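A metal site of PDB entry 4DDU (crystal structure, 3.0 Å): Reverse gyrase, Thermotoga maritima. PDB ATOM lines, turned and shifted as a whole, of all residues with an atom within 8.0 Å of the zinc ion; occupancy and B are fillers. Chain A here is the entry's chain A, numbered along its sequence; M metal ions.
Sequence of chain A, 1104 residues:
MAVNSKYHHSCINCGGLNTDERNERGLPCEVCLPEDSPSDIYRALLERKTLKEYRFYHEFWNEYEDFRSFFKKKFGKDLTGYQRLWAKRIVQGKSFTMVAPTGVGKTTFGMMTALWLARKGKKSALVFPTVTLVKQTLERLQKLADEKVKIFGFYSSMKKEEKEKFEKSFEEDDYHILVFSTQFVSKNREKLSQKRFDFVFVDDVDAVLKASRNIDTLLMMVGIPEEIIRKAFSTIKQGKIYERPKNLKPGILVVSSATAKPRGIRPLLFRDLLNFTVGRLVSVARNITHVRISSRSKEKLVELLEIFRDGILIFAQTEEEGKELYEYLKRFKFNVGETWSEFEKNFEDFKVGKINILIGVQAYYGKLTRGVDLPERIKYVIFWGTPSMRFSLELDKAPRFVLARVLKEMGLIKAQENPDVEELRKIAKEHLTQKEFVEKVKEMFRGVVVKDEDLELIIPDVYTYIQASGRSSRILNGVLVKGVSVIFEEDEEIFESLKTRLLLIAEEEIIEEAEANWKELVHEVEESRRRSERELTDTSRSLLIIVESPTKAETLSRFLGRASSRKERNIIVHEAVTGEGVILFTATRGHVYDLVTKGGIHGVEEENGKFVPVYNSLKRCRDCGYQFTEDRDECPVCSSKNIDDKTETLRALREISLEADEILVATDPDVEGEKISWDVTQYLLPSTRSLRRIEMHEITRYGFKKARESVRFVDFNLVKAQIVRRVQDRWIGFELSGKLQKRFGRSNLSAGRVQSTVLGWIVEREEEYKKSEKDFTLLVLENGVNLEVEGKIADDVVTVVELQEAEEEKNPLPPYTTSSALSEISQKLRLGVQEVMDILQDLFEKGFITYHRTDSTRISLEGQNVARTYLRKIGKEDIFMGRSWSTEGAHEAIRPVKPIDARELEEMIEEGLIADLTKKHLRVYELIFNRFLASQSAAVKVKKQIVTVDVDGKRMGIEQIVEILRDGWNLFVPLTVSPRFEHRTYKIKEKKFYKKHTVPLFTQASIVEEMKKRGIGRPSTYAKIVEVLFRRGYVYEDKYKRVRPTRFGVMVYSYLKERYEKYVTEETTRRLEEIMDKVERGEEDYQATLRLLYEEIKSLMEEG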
ATOM      1  N   SER A  10      37.189 -14.302  26.857  1.00  0.00           N
ATOM      2  CA  SER A  10      36.837 -14.034  28.244  1.00  0.00           C
ATOM      3  C   SER A  10      35.418 -13.522  28.446  1.00  0.00           C
ATOM      4  O   SER A  10      35.054 -13.147  29.556  1.00  0.00           O
ATOM      5  CB  SER A  10      37.829 -13.051  28.841  1.00  0.00           C
ATOM      6  OG  SER A  10      37.871 -11.846  28.085  1.00  0.00           O
ATOM      7  N   CYS A  11      34.625 -13.486  27.385  1.00  0.00           N
ATOM      8  CA  CYS A  11      33.240 -13.051  27.528  1.00  0.00           C
ATOM      9  C   CYS A  11      32.385 -14.185  28.079  1.00  0.00           C
ATOM     10  O   CYS A  11      32.340 -15.281  27.503  1.00  0.00           O
ATOM     11  CB  CYS A  11      32.650 -12.520  26.232  1.00  0.00           C
ATOM     12  SG  CYS A  11      31.037 -11.723  26.462  1.00  0.00           S
ATOM     13  N   ILE A  12      31.719 -13.904  29.190  1.00  0.00           N
ATOM     14  CA  ILE A  12      30.910 -14.897  29.873  1.00  0.00           C
ATOM     15  C   ILE A  12      29.724 -15.341  29.010  1.00  0.00           C
ATOM     16  O   ILE A  12      29.227 -16.456  29.158  1.00  0.00           O
ATOM     17  CB  ILE A  12      30.417 -14.342  31.226  1.00  0.00           C
ATOM     18  CG1 ILE A  12      29.717 -15.434  32.056  1.00  0.00           C
ATOM     19  CG2 ILE A  12      29.545 -13.114  31.033  1.00  0.00           C
ATOM     20  CD1 ILE A  12      30.651 -16.490  32.594  1.00  0.00           C
ATOM     21  N   ASN A  13      29.313 -14.470  28.084  1.00  0.00           N
ATOM     22  CA  ASN A  13      28.065 -14.669  27.347  1.00  0.00           C
ATOM     23  C   ASN A  13      28.192 -14.988  25.842  1.00  0.00           C
ATOM     24  O   ASN A  13      27.515 -15.880  25.348  1.00  0.00           O
ATOM     25  CB  ASN A  13      27.148 -13.460  27.546  1.00  0.00           C
ATOM     26  CG  ASN A  13      25.984 -13.450  26.592  1.00  0.00           C
ATOM     27  OD1 ASN A  13      25.000 -14.173  26.781  1.00  0.00           O
ATOM     28  ND2 ASN A  13      26.055 -12.616  25.574  1.00  0.00           N
ATOM     29  N   CYS A  14      29.040 -14.259  25.121  1.00  0.00           N
ATOM     30  CA  CYS A  14      29.213 -14.511  23.690  1.00  0.00           C
ATOM     31  C   CYS A  14      30.368 -15.459  23.417  1.00  0.00           C
ATOM     32  O   CYS A  14      30.500 -16.000  22.315  1.00  0.00           O
ATOM     33  CB  CYS A  14      29.355 -13.202  22.892  1.00  0.00           C
ATOM     34  SG  CYS A  14      30.989 -12.402  22.926  1.00  0.00           S
ATOM     35  N   GLY A  15      31.212 -15.663  24.434  1.00  0.00           N
ATOM     36  CA  GLY A  15      32.330 -16.580  24.323  1.00  0.00           C
ATOM     37  C   GLY A  15      33.496 -16.003  23.558  1.00  0.00           C
ATOM     38  O   GLY A  15      34.371 -16.735  23.093  1.00  0.00           O
ATOM     39  N   GLY A  16      33.535 -14.677  23.432  1.00  0.00           N
ATOM     40  CA  GLY A  16      34.563 -14.009  22.666  1.00  0.00           C
ATOM     41  C   GLY A  16      35.394 -13.013  23.456  1.00  0.00           C
ATOM     42  O   GLY A  16      35.442 -13.045  24.688  1.00  0.00           O
ATOM     43  N   LEU A  17      36.057 -12.115  22.726  1.00  0.00           N
ATOM     44  CA  LEU A  17      36.951 -11.130  23.318  1.00  0.00           C
ATOM     45  C   LEU A  17      36.255 -10.143  24.268  1.00  0.00           C
ATOM     46  O   LEU A  17      35.185  -9.624  23.969  1.00  0.00           O
ATOM     47  CB  LEU A  17      37.670 -10.369  22.206  1.00  0.00           C
ATOM     48  CG  LEU A  17      38.581  -9.195  22.597  1.00  0.00           C
ATOM     49  CD1 LEU A  17      39.872  -9.277  21.812  1.00  0.00           C
ATOM     50  CD2 LEU A  17      37.873  -7.866  22.352  1.00  0.00           C
ATOM     51  N   ASN A  18      36.896  -9.886  25.406  1.00  0.00           N
ATOM     52  CA  ASN A  18      36.439  -8.873  26.356  1.00  0.00           C
ATOM     53  C   ASN A  18      37.633  -8.223  27.043  1.00  0.00           C
ATOM     54  O   ASN A  18      38.707  -8.812  27.105  1.00  0.00           O
ATOM     55  CB  ASN A  18      35.500  -9.467  27.408  1.00  0.00           C
ATOM     56  CG  ASN A  18      34.856  -8.400  28.280  1.00  0.00           C
ATOM     57  OD1 ASN A  18      34.853  -7.220  27.941  1.00  0.00           O
ATOM     58  ND2 ASN A  18      34.301  -8.821  29.407  1.00  0.00           N
ATOM     59  N   LEU A  27      31.166  -8.378  33.899  1.00  0.00           N
ATOM     60  CA  LEU A  27      30.319  -7.971  32.790  1.00  0.00           C
ATOM     61  C   LEU A  27      30.691  -8.675  31.494  1.00  0.00           C
ATOM     62  O   LEU A  27      31.841  -9.085  31.313  1.00  0.00           O
ATOM     63  CB  LEU A  27      30.406  -6.452  32.595  1.00  0.00           C
ATOM     64  CG  LEU A  27      29.887  -5.603  33.746  1.00  0.00           C
ATOM     65  CD1 LEU A  27      29.999  -4.126  33.408  1.00  0.00           C
ATOM     66  CD2 LEU A  27      28.450  -5.964  34.059  1.00  0.00           C
ATOM     67  N   PRO A  28      29.712  -8.835  30.588  1.00  0.00           N
ATOM     68  CA  PRO A  28      29.980  -9.306  29.231  1.00  0.00           C
ATOM     69  C   PRO A  28      30.566  -8.170  28.406  1.00  0.00           C
ATOM     70  O   PRO A  28      30.527  -7.018  28.855  1.00  0.00           O
ATOM     71  CB  PRO A  28      28.599  -9.687  28.702  1.00  0.00           C
ATOM     72  CG  PRO A  28      27.716  -9.769  29.918  1.00  0.00           C
ATOM     73  CD  PRO A  28      28.265  -8.775  30.873  1.00  0.00           C
ATOM     74  N   CYS A  29      31.085  -8.474  27.218  1.00  0.00           N
ATOM     75  CA  CYS A  29      31.738  -7.469  26.373  1.00  0.00           C
ATOM     76  C   CYS A  29      30.792  -6.347  25.962  1.00  0.00           C
ATOM     77  O   CYS A  29      29.591  -6.418  26.199  1.00  0.00           O
ATOM     78  CB  CYS A  29      32.346  -8.124  25.136  1.00  0.00           C
ATOM     79  SG  CYS A  29      31.146  -8.806  23.977  1.00  0.00           S
ATOM     80  N   GLU A  30      31.340  -5.294  25.357  1.00  0.00           N
ATOM     81  CA  GLU A  30      30.523  -4.168  24.920  1.00  0.00           C
ATOM     82  C   GLU A  30      29.630  -4.534  23.742  1.00  0.00           C
ATOM     83  O   GLU A  30      28.566  -3.941  23.560  1.00  0.00           O
ATOM     84  CB  GLU A  30      31.391  -2.953  24.559  1.00  0.00           C
ATOM     85  CG  GLU A  30      31.665  -2.020  25.719  1.00  0.00           C
ATOM     86  CD  GLU A  30      33.091  -2.124  26.219  1.00  0.00           C
ATOM     87  OE1 GLU A  30      33.676  -3.226  26.175  1.00  0.00           O
ATOM     88  OE2 GLU A  30      33.634  -1.084  26.648  1.00  0.00           O
ATOM     89  N   VAL A  31      30.061  -5.514  22.946  1.00  0.00           N
ATOM     90  CA  VAL A  31      29.245  -6.028  21.849  1.00  0.00           C
ATOM     91  C   VAL A  31      27.944  -6.614  22.405  1.00  0.00           C
ATOM     92  O   VAL A  31      26.859  -6.285  21.950  1.00  0.00           O
ATOM     93  CB  VAL A  31      29.987  -7.116  21.040  1.00  0.00           C
ATOM     94  CG1 VAL A  31      29.027  -7.865  20.132  1.00  0.00           C
ATOM     95  CG2 VAL A  31      31.108  -6.503  20.229  1.00  0.00           C
ATOM     96  N   CYS A  32      28.085  -7.469  23.416  1.00  0.00           N
ATOM     97  CA  CYS A  32      26.937  -8.110  24.037  1.00  0.00           C
ATOM     98  C   CYS A  32      26.061  -7.116  24.790  1.00  0.00           C
ATOM     99  O   CYS A  32      24.849  -7.303  24.901  1.00  0.00           O
ATOM    100  CB  CYS A  32      27.395  -9.215  24.990  1.00  0.00           C
ATOM    101  SG  CYS A  32      27.985 -10.715  24.188  1.00  0.00           S
ATOM    102  N   LEU A  33      26.675  -6.055  25.300  1.00  0.00           N
ATOM    103  CA  LEU A  33      25.990  -5.156  26.219  1.00  0.00           C
ATOM    104  C   LEU A  33      26.686  -3.809  26.296  1.00  0.00           C
ATOM    105  O   LEU A  33      27.448  -3.550  27.222  1.00  0.00           O
ATOM    106  CB  LEU A  33      25.924  -5.802  27.601  1.00  0.00           C
ATOM    107  CG  LEU A  33      25.030  -5.151  28.663  1.00  0.00           C
ATOM    108  CD1 LEU A  33      23.610  -5.055  28.157  1.00  0.00           C
ATOM    109  CD2 LEU A  33      25.102  -5.965  29.937  1.00  0.00           C
ATOM    110  N   LEU A  45      20.704  -8.346  28.873  1.00  0.00           N
ATOM    111  CA  LEU A  45      21.073  -9.186  27.731  1.00  0.00           C
ATOM    112  C   LEU A  45      19.829  -9.564  26.953  1.00  0.00           C
ATOM    113  O   LEU A  45      19.833  -9.550  25.718  1.00  0.00           O
ATOM    114  CB  LEU A  45      21.789 -10.443  28.205  1.00  0.00           C
ATOM    115  CG  LEU A  45      23.266 -10.309  28.570  1.00  0.00           C
ATOM    116  CD1 LEU A  45      23.787 -11.618  29.081  1.00  0.00           C
ATOM    117  CD2 LEU A  45      24.073  -9.845  27.363  1.00  0.00           C
ATOM    118  N   THR A  50      20.809 -10.167  22.954  1.00  0.00           N
ATOM    119  CA  THR A  50      22.157 -10.712  22.794  1.00  0.00           C
ATOM    120  C   THR A  50      22.410 -11.851  23.771  1.00  0.00           C
ATOM    121  O   THR A  50      23.533 -12.336  23.903  1.00  0.00           O
ATOM    122  CB  THR A  50      23.234  -9.628  22.978  1.00  0.00           C
ATOM    123  OG1 THR A  50      22.850  -8.738  24.031  1.00  0.00           O
ATOM    124  CG2 THR A  50      23.422  -8.833  21.702  1.00  0.00           C
ATOM    125  N   LYS A  52      23.012 -15.210  25.106  1.00  0.00           N
ATOM    126  CA  LYS A  52      23.427 -16.515  24.596  1.00  0.00           C
ATOM    127  C   LYS A  52      23.792 -17.498  25.715  1.00  0.00           C
ATOM    128  O   LYS A  52      22.933 -18.204  26.235  1.00  0.00           O
ATOM    129  CB  LYS A  52      24.607 -16.359  23.629  1.00  0.00           C
ATOM    130  CG  LYS A  52      24.993 -17.637  22.883  1.00  0.00           C
ATOM    131  CD  LYS A  52      26.207 -17.414  21.998  1.00  0.00           C
ATOM    132  CE  LYS A  52      26.675 -18.705  21.342  1.00  0.00           C
ATOM    133  NZ  LYS A  52      27.940 -18.508  20.590  1.00  0.00           N
HETATM  134 ZN    ZN M   1      30.195 -10.841  24.397  1.00  0.00          ZN
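O of Gly 16 is in hydrogen-bond range of N of Cys 11 (2.9 Å). The side-chain sulfur of Cys 14 lies close to the backbone NH of Gly 16. The backbone NH (N) of Val 31 lies close to the side-chain sulfur (SG) of Cys 29 (3.6 Å). SG of Cys 32 sits close to ND2 of Asn 13, at 3.0 Å. O of Cys 32 is in hydrogen-bond range of OG1 of Thr 50. The side-chain sulfur of Cys 11 lies close to the backbone NH of Asn 13 (3.6 Å).
Of the 19 residues printed, 4 come within 4 Å of the zinc ion. Along chain A the residues within 4 Å of the zinc ion span positions 11 to 32.
The zinc ion is bound by SG of Cys 32 (2.2 Å), SG of Cys 29 (2.3 Å), SG of Cys 14 (2.3 Å) and SG of Cys 11 (2.4 Å).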
